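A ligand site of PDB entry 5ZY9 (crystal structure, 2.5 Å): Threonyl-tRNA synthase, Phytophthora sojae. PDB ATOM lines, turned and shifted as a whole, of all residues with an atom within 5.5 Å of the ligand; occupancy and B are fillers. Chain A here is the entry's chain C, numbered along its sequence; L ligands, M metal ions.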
ATOM      1  N   SER A  66      12.769 -27.048  14.576  1.00  0.00           N
ATOM      2  CA  SER A  66      12.581 -25.644  14.820  1.00  0.00           C
ATOM      3  C   SER A  66      11.142 -25.214  15.126  1.00  0.00           C
ATOM      4  O   SER A  66      10.924 -24.256  15.805  1.00  0.00           O
ATOM      5  CB  SER A  66      13.189 -24.827  13.729  1.00  0.00           C
ATOM      6  OG  SER A  66      12.691 -25.209  12.502  1.00  0.00           O
ATOM      7  N   GLY A  67      10.180 -25.972  14.634  1.00  0.00           N
ATOM      8  CA  GLY A  67       8.803 -25.601  14.642  1.00  0.00           C
ATOM      9  C   GLY A  67       8.266 -25.138  13.313  1.00  0.00           C
ATOM     10  O   GLY A  67       7.098 -24.976  13.172  1.00  0.00           O
ATOM     11  N   HIS A  68       9.131 -24.973  12.342  1.00  0.00           N
ATOM     12  CA  HIS A  68       8.754 -24.522  11.037  1.00  0.00           C
ATOM     13  C   HIS A  68       7.858 -25.464  10.349  1.00  0.00           C
ATOM     14  O   HIS A  68       6.972 -25.046   9.684  1.00  0.00           O
ATOM     15  CB  HIS A  68       9.960 -24.172  10.191  1.00  0.00           C
ATOM     16  CG  HIS A  68      10.602 -22.886  10.587  1.00  0.00           C
ATOM     17  ND1 HIS A  68      11.638 -22.835  11.472  1.00  0.00           N
ATOM     18  CD2 HIS A  68      10.320 -21.614  10.261  1.00  0.00           C
ATOM     19  CE1 HIS A  68      11.977 -21.583  11.663  1.00  0.00           C
ATOM     20  NE2 HIS A  68      11.192 -20.824  10.941  1.00  0.00           N
ATOM     21  N   HIS A  71       4.355 -24.822  12.046  1.00  0.00           N
ATOM     22  CA  HIS A  71       3.872 -23.483  11.893  1.00  0.00           C
ATOM     23  C   HIS A  71       4.047 -22.790  10.572  1.00  0.00           C
ATOM     24  O   HIS A  71       3.377 -21.852  10.344  1.00  0.00           O
ATOM     25  CB  HIS A  71       4.487 -22.616  12.944  1.00  0.00           C
ATOM     26  CG  HIS A  71       4.152 -23.029  14.341  1.00  0.00           C
ATOM     27  ND1 HIS A  71       2.859 -23.202  14.765  1.00  0.00           N
ATOM     28  CD2 HIS A  71       4.927 -23.274  15.401  1.00  0.00           C
ATOM     29  CE1 HIS A  71       2.867 -23.555  16.034  1.00  0.00           C
ATOM     30  NE2 HIS A  71       4.109 -23.603  16.434  1.00  0.00           N
ATOM     31  N   TYR A  72       5.003 -23.189   9.768  1.00  0.00           N
ATOM     32  CA  TYR A  72       5.387 -22.381   8.625  1.00  0.00           C
ATOM     33  C   TYR A  72       5.419 -23.033   7.284  1.00  0.00           C
ATOM     34  O   TYR A  72       5.793 -22.430   6.362  1.00  0.00           O
ATOM     35  CB  TYR A  72       6.753 -21.828   8.888  1.00  0.00           C
ATOM     36  CG  TYR A  72       6.903 -20.412   8.556  1.00  0.00           C
ATOM     37  CD1 TYR A  72       6.394 -19.447   9.356  1.00  0.00           C
ATOM     38  CD2 TYR A  72       7.567 -20.031   7.440  1.00  0.00           C
ATOM     39  CE1 TYR A  72       6.536 -18.141   9.042  1.00  0.00           C
ATOM     40  CE2 TYR A  72       7.694 -18.728   7.107  1.00  0.00           C
ATOM     41  CZ  TYR A  72       7.184 -17.785   7.915  1.00  0.00           C
ATOM     42  OH  TYR A  72       7.336 -16.497   7.579  1.00  0.00           O
ATOM     43  N   MET A  91      14.010 -18.733   7.235  1.00  0.00           N
ATOM     44  CA  MET A  91      14.743 -18.038   8.276  1.00  0.00           C
ATOM     45  C   MET A  91      16.137 -18.612   8.513  1.00  0.00           C
ATOM     46  O   MET A  91      16.386 -19.746   8.263  1.00  0.00           O
ATOM     47  CB  MET A  91      13.948 -18.088   9.570  1.00  0.00           C
ATOM     48  CG  MET A  91      12.662 -17.307   9.585  1.00  0.00           C
ATOM     49  SD  MET A  91      11.741 -17.292  11.092  1.00  0.00           S
ATOM     50  CE  MET A  91      10.222 -16.539  10.630  1.00  0.00           C
ATOM     51  N   CYS A  93      17.407 -18.392  11.518  1.00  0.00           N
ATOM     52  CA  CYS A  93      17.401 -18.379  12.958  1.00  0.00           C
ATOM     53  C   CYS A  93      17.864 -19.892  13.403  1.00  0.00           C
ATOM     54  O   CYS A  93      18.736 -20.077  14.242  1.00  0.00           O
ATOM     55  CB  CYS A  93      16.031 -18.015  13.527  1.00  0.00           C
ATOM     56  SG  CYS A  93      15.049 -16.927  12.471  1.00  0.00           S
ATOM     57  N   PRO A  94      17.401 -20.968  12.788  1.00  0.00           N
ATOM     58  CA  PRO A  94      17.906 -22.331  13.074  1.00  0.00           C
ATOM     59  C   PRO A  94      19.339 -22.785  12.735  1.00  0.00           C
ATOM     60  O   PRO A  94      19.893 -23.589  13.429  1.00  0.00           O
ATOM     61  CB  PRO A  94      16.907 -23.246  12.370  1.00  0.00           C
ATOM     62  CG  PRO A  94      15.785 -22.390  12.043  1.00  0.00           C
ATOM     63  CD  PRO A  94      16.306 -21.025  11.824  1.00  0.00           C
ATOM     64  N   ARG A 122      10.140 -17.218   0.939  1.00  0.00           N
ATOM     65  CA  ARG A 122       8.887 -17.512   1.561  1.00  0.00           C
ATOM     66  C   ARG A 122       7.902 -17.634   0.457  1.00  0.00           C
ATOM     67  O   ARG A 122       7.953 -16.906  -0.451  1.00  0.00           O
ATOM     68  CB  ARG A 122       8.510 -16.447   2.577  1.00  0.00           C
ATOM     69  CG  ARG A 122       9.166 -16.683   3.914  1.00  0.00           C
ATOM     70  CD  ARG A 122       9.180 -15.499   4.787  1.00  0.00           C
ATOM     71  NE  ARG A 122      10.259 -15.501   5.726  1.00  0.00           N
ATOM     72  CZ  ARG A 122      10.321 -14.749   6.811  1.00  0.00           C
ATOM     73  NH1 ARG A 122       9.357 -13.954   7.100  1.00  0.00           N
ATOM     74  NH2 ARG A 122      11.354 -14.798   7.578  1.00  0.00           N
ATOM     75  N   GLN A 140      17.610 -10.479   4.782  1.00  0.00           N
ATOM     76  CA  GLN A 140      17.490  -9.759   6.011  1.00  0.00           C
ATOM     77  C   GLN A 140      18.803  -9.337   6.547  1.00  0.00           C
ATOM     78  O   GLN A 140      19.774  -9.963   6.324  1.00  0.00           O
ATOM     79  CB  GLN A 140      16.820 -10.610   7.054  1.00  0.00           C
ATOM     80  CG  GLN A 140      15.363 -10.814   6.893  1.00  0.00           C
ATOM     81  CD  GLN A 140      14.814 -11.786   7.889  1.00  0.00           C
ATOM     82  OE1 GLN A 140      15.536 -12.447   8.545  1.00  0.00           O
ATOM     83  NE2 GLN A 140      13.533 -11.847   7.995  1.00  0.00           N
ATOM     84  N   ASP A 142      19.649  -9.985   9.439  1.00  0.00           N
ATOM     85  CA  ASP A 142      19.462 -10.839  10.581  1.00  0.00           C
ATOM     86  C   ASP A 142      20.705 -10.955  11.388  1.00  0.00           C
ATOM     87  O   ASP A 142      21.754 -11.025  10.871  1.00  0.00           O
ATOM     88  CB  ASP A 142      19.103 -12.219  10.060  1.00  0.00           C
ATOM     89  CG  ASP A 142      18.208 -12.993  10.986  1.00  0.00           C
ATOM     90  OD1 ASP A 142      17.717 -12.509  11.988  1.00  0.00           O
ATOM     91  OD2 ASP A 142      17.952 -14.126  10.653  1.00  0.00           O
ATOM     92  N   ALA A 220       5.062 -13.342  21.703  1.00  0.00           N
ATOM     93  CA  ALA A 220       5.074 -14.592  21.014  1.00  0.00           C
ATOM     94  C   ALA A 220       5.017 -15.689  22.017  1.00  0.00           C
ATOM     95  O   ALA A 220       5.391 -15.501  23.114  1.00  0.00           O
ATOM     96  CB  ALA A 220       6.317 -14.696  20.175  1.00  0.00           C
ATOM     97  N   PHE A 221       4.566 -16.835  21.602  1.00  0.00           N
ATOM     98  CA  PHE A 221       4.506 -17.969  22.471  1.00  0.00           C
ATOM     99  C   PHE A 221       5.870 -18.355  22.986  1.00  0.00           C
ATOM    100  O   PHE A 221       5.981 -18.850  24.053  1.00  0.00           O
ATOM    101  CB  PHE A 221       3.740 -19.133  21.859  1.00  0.00           C
ATOM    102  CG  PHE A 221       4.429 -19.850  20.740  1.00  0.00           C
ATOM    103  CD1 PHE A 221       5.443 -20.731  20.981  1.00  0.00           C
ATOM    104  CD2 PHE A 221       4.001 -19.697  19.476  1.00  0.00           C
ATOM    105  CE1 PHE A 221       6.023 -21.395  19.966  1.00  0.00           C
ATOM    106  CE2 PHE A 221       4.581 -20.361  18.461  1.00  0.00           C
ATOM    107  CZ  PHE A 221       5.588 -21.213  18.696  1.00  0.00           C
ATOM    108  N   TYR A 222       6.891 -18.084  22.207  1.00  0.00           N
ATOM    109  CA  TYR A 222       8.242 -18.409  22.579  1.00  0.00           C
ATOM    110  C   TYR A 222       9.046 -17.278  23.180  1.00  0.00           C
ATOM    111  O   TYR A 222      10.135 -17.497  23.589  1.00  0.00           O
ATOM    112  CB  TYR A 222       8.981 -18.997  21.393  1.00  0.00           C
ATOM    113  CG  TYR A 222       8.827 -18.149  20.186  1.00  0.00           C
ATOM    114  CD1 TYR A 222       9.662 -17.116  19.974  1.00  0.00           C
ATOM    115  CD2 TYR A 222       7.795 -18.333  19.333  1.00  0.00           C
ATOM    116  CE1 TYR A 222       9.491 -16.301  18.920  1.00  0.00           C
ATOM    117  CE2 TYR A 222       7.615 -17.530  18.265  1.00  0.00           C
ATOM    118  CZ  TYR A 222       8.494 -16.506  18.076  1.00  0.00           C
ATOM    119  OH  TYR A 222       8.364 -15.687  17.053  1.00  0.00           O
ATOM    120  N   LYS A 225       8.818  -9.587  23.114  1.00  0.00           N
ATOM    121  CA  LYS A 225       9.471  -8.806  22.103  1.00  0.00           C
ATOM    122  C   LYS A 225       9.299  -7.332  22.301  1.00  0.00           C
ATOM    123  O   LYS A 225       8.401  -6.925  22.948  1.00  0.00           O
ATOM    124  CB  LYS A 225       8.972  -9.203  20.720  1.00  0.00           C
ATOM    125  CG  LYS A 225       7.516  -8.934  20.476  1.00  0.00           C
ATOM    126  CD  LYS A 225       7.174  -9.344  19.089  1.00  0.00           C
ATOM    127  CE  LYS A 225       5.741  -9.117  18.743  1.00  0.00           C
ATOM    128  NZ  LYS A 225       5.521  -9.560  17.363  1.00  0.00           N
ATOM    129  N   THR A 242      13.147  -5.254  14.844  1.00  0.00           N
ATOM    130  CA  THR A 242      12.540  -6.008  15.905  1.00  0.00           C
ATOM    131  C   THR A 242      13.531  -6.524  16.917  1.00  0.00           C
ATOM    132  O   THR A 242      14.649  -6.620  16.642  1.00  0.00           O
ATOM    133  CB  THR A 242      11.704  -7.146  15.379  1.00  0.00           C
ATOM    134  OG1 THR A 242      11.209  -7.898  16.484  1.00  0.00           O
ATOM    135  CG2 THR A 242      12.499  -8.020  14.507  1.00  0.00           C
ATOM    136  N   GLN A 244      13.333  -9.790  19.438  1.00  0.00           N
ATOM    137  CA  GLN A 244      12.468 -10.849  19.855  1.00  0.00           C
ATOM    138  C   GLN A 244      13.282 -11.862  20.551  1.00  0.00           C
ATOM    139  O   GLN A 244      14.129 -12.438  19.979  1.00  0.00           O
ATOM    140  CB  GLN A 244      11.850 -11.460  18.605  1.00  0.00           C
ATOM    141  CG  GLN A 244      11.078 -12.744  18.767  1.00  0.00           C
ATOM    142  CD  GLN A 244       9.774 -12.605  19.491  1.00  0.00           C
ATOM    143  OE1 GLN A 244       8.799 -12.213  18.929  1.00  0.00           O
ATOM    144  NE2 GLN A 244       9.765 -12.925  20.740  1.00  0.00           N
ATOM    145  N   ASP A 246      13.680 -15.542  22.413  1.00  0.00           N
ATOM    146  CA  ASP A 246      13.224 -16.854  22.145  1.00  0.00           C
ATOM    147  C   ASP A 246      13.675 -17.761  23.260  1.00  0.00           C
ATOM    148  O   ASP A 246      14.823 -17.828  23.543  1.00  0.00           O
ATOM    149  CB  ASP A 246      13.846 -17.289  20.848  1.00  0.00           C
ATOM    150  CG  ASP A 246      13.125 -18.358  20.221  1.00  0.00           C
ATOM    151  OD1 ASP A 246      12.638 -19.216  20.893  1.00  0.00           O
ATOM    152  OD2 ASP A 246      13.063 -18.371  19.032  1.00  0.00           O
ATOM    153  N   GLN A 248      12.269 -20.962  23.240  1.00  0.00           N
ATOM    154  CA  GLN A 248      12.048 -22.242  22.650  1.00  0.00           C
ATOM    155  C   GLN A 248      13.204 -22.734  21.825  1.00  0.00           C
ATOM    156  O   GLN A 248      13.643 -23.825  22.006  1.00  0.00           O
ATOM    157  CB  GLN A 248      10.761 -22.314  21.867  1.00  0.00           C
ATOM    158  CG  GLN A 248      10.571 -23.701  21.312  1.00  0.00           C
ATOM    159  CD  GLN A 248       9.320 -23.909  20.543  1.00  0.00           C
ATOM    160  OE1 GLN A 248       9.337 -24.200  19.394  1.00  0.00           O
ATOM    161  NE2 GLN A 248       8.235 -23.786  21.205  1.00  0.00           N
ATOM    162  N   LEU A 249      13.605 -21.810  20.948  1.00  0.00           N
ATOM    163  CA  LEU A 249      14.771 -21.884  20.104  1.00  0.00           C
ATOM    164  C   LEU A 249      15.909 -22.535  20.830  1.00  0.00           C
ATOM    165  O   LEU A 249      16.527 -23.443  20.273  1.00  0.00           O
ATOM    166  CB  LEU A 249      15.168 -20.485  19.629  1.00  0.00           C
ATOM    167  CG  LEU A 249      16.187 -20.423  18.492  1.00  0.00           C
ATOM    168  CD1 LEU A 249      17.048 -21.677  18.470  1.00  0.00           C
ATOM    169  CD2 LEU A 249      15.501 -20.218  17.159  1.00  0.00           C
ATOM    170  N   HIS A 272      16.517 -12.739  18.366  1.00  0.00           N
ATOM    171  CA  HIS A 272      16.482 -12.570  16.919  1.00  0.00           C
ATOM    172  C   HIS A 272      16.210 -11.111  16.595  1.00  0.00           C
ATOM    173  O   HIS A 272      15.096 -10.617  16.795  1.00  0.00           O
ATOM    174  CB  HIS A 272      15.398 -13.464  16.303  1.00  0.00           C
ATOM    175  CG  HIS A 272      15.364 -14.851  16.884  1.00  0.00           C
ATOM    176  ND1 HIS A 272      15.564 -15.974  16.111  1.00  0.00           N
ATOM    177  CD2 HIS A 272      15.135 -15.277  18.141  1.00  0.00           C
ATOM    178  CE1 HIS A 272      15.472 -17.048  16.883  1.00  0.00           C
ATOM    179  NE2 HIS A 272      15.207 -16.656  18.110  1.00  0.00           N
ATOM    180  N   ALA A 274      16.780  -7.364  14.095  1.00  0.00           N
ATOM    181  CA  ALA A 274      16.949  -6.723  12.797  1.00  0.00           C
ATOM    182  C   ALA A 274      16.766  -5.223  12.853  1.00  0.00           C
ATOM    183  O   ALA A 274      16.194  -4.740  13.772  1.00  0.00           O
ATOM    184  CB  ALA A 274      16.039  -7.325  11.761  1.00  0.00           C
HETATM  185  C1  LIG L   1      11.175 -12.833  13.022  1.00  0.00           C
HETATM  186  C2  LIG L   1      10.490 -12.044  11.952  1.00  0.00           C
HETATM  187  C3  LIG L   1      11.308 -10.810  11.743  1.00  0.00           C
HETATM  188  C4  LIG L   1      12.703 -11.125  12.245  1.00  0.00           C
HETATM  189  C5  LIG L   1      12.469 -12.091  13.388  1.00  0.00           C
HETATM  190  C6  LIG L   1      10.362 -13.297  14.229  1.00  0.00           C
HETATM  191  C7  LIG L   1      11.407 -13.991  15.110  1.00  0.00           C
HETATM  192  C8  LIG L   1      11.396 -15.502  15.420  1.00  0.00           C
HETATM  193  C9  LIG L   1      12.043 -16.467  14.804  1.00  0.00           C
HETATM  194  C10 LIG L   1      11.771 -17.717  15.467  1.00  0.00           C
HETATM  195  C11 LIG L   1      11.994 -19.056  15.509  1.00  0.00           C
HETATM  196  C12 LIG L   1      12.734 -19.876  14.920  1.00  0.00           C
HETATM  197  C13 LIG L   1      11.136 -19.616  16.639  1.00  0.00           C
HETATM  198  C14 LIG L   1      10.066 -20.521  16.100  1.00  0.00           C
HETATM  199  C15 LIG L   1       9.185 -21.082  17.246  1.00  0.00           C
HETATM  200  C16 LIG L   1       9.267 -19.732  15.079  1.00  0.00           C
HETATM  201  C17 LIG L   1       8.089 -20.482  14.513  1.00  0.00           C
HETATM  202  C18 LIG L   1       8.552 -21.762  13.784  1.00  0.00           C
HETATM  203  C19 LIG L   1       7.233 -19.639  13.527  1.00  0.00           C
HETATM  204  C20 LIG L   1       6.464 -18.427  14.102  1.00  0.00           C
HETATM  205  C21 LIG L   1       5.466 -18.894  15.147  1.00  0.00           C
HETATM  206  C22 LIG L   1       5.787 -17.651  12.961  1.00  0.00           C
HETATM  207  C23 LIG L   1       5.103 -16.350  13.374  1.00  0.00           C
HETATM  208  C24 LIG L   1       4.378 -15.775  12.179  1.00  0.00           C
HETATM  209  C25 LIG L   1       6.071 -15.313  13.950  1.00  0.00           C
HETATM  210  C26 LIG L   1       7.416 -15.283  13.174  1.00  0.00           C
HETATM  211  C27 LIG L   1       8.240 -14.252  13.889  1.00  0.00           C
HETATM  212  O1  LIG L   1       7.807 -13.484  14.671  1.00  0.00           O
HETATM  213  O2  LIG L   1       9.603 -14.258  13.604  1.00  0.00           O
HETATM  214  C28 LIG L   1      10.534 -12.736  10.624  1.00  0.00           C
HETATM  215  O3  LIG L   1       9.467 -12.815   9.943  1.00  0.00           O
HETATM  216  O4  LIG L   1      11.630 -13.224  10.212  1.00  0.00           O
HETATM  217  O5  LIG L   1      11.904 -20.139  17.706  1.00  0.00           O
HETATM  218  O6  LIG L   1       6.341 -15.730  15.282  1.00  0.00           O
HETATM  219  N1  LIG L   1      13.499 -20.714  14.564  1.00  0.00           N
HETATM  220 ZN    ZN M   1      15.292 -15.724  14.179  1.00  0.00          ZN
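O5 of the ligand sits at hydrogen-bond distance from OD2 of Asp 246, at 2.5 Å.
An oxygen (O3) of the ligand is in salt-bridge range of the guanidinium group (NH1) of Arg 122.
O4 of the ligand sits at hydrogen-bond distance from NE2 of Gln 140 (3.2 Å).
O6 of the ligand sits at hydrogen-bond distance from OH of Tyr 222 (2.7 Å).
The side-chain carboxylate of Asp 246 is in hydrogen-bond range of a ring nitrogen (NE2) of His 272, at 2.9 Å.
OD1 of Asp 246 sits at hydrogen-bond distance from N of Gln 248.
The side-chain hydroxyl (OG) of Ser 66 is in hydrogen-bond range of a ring nitrogen (ND1) of His 68, 2.8 Å away.
The backbone NH (N) of His 272 sits at hydrogen-bond distance from the backbone carbonyl oxygen (O) of Gln 244 (2.9 Å).
The guanidinium group of Arg 122 lies within hydrogen-bond range of the side-chain hydroxyl of Tyr 72 (3.3 Å).
OD1 of Asp 246 lies within hydrogen-bond range of N of Leu 249 (2.8 Å).
O of Ala 274 lies within hydrogen-bond range of N of Thr 242.
The side-chain sulfur (SG) of Cys 93 sits close to the side-chain sulfur (SD) of Met 91 (3.6 Å).
Merely in contact with the ligand: Ser 66 (3.8 Å), Gly 67 (3.4 Å), His 68 (3.4 Å), Met 91 (3.6 Å), Cys 93 (3.8 Å), Pro 94 (3.8 Å), Phe 221 (3.7 Å), Thr 242 (3.8 Å), Gln 244 (3.9 Å), Gln 248 (3.8 Å), Leu 249 (3.3 Å) and His 272 (3.8 Å).
Hydrophobic or aromatic side chains that line the ligand: His 68, Met 91, Pro 94, Phe 221, Tyr 222 and Leu 249.
Of the 22 residues printed, 16 come within 4 Å of the ligand.
Along chain A the residues within 4 Å of the ligand span positions 66 to 272.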
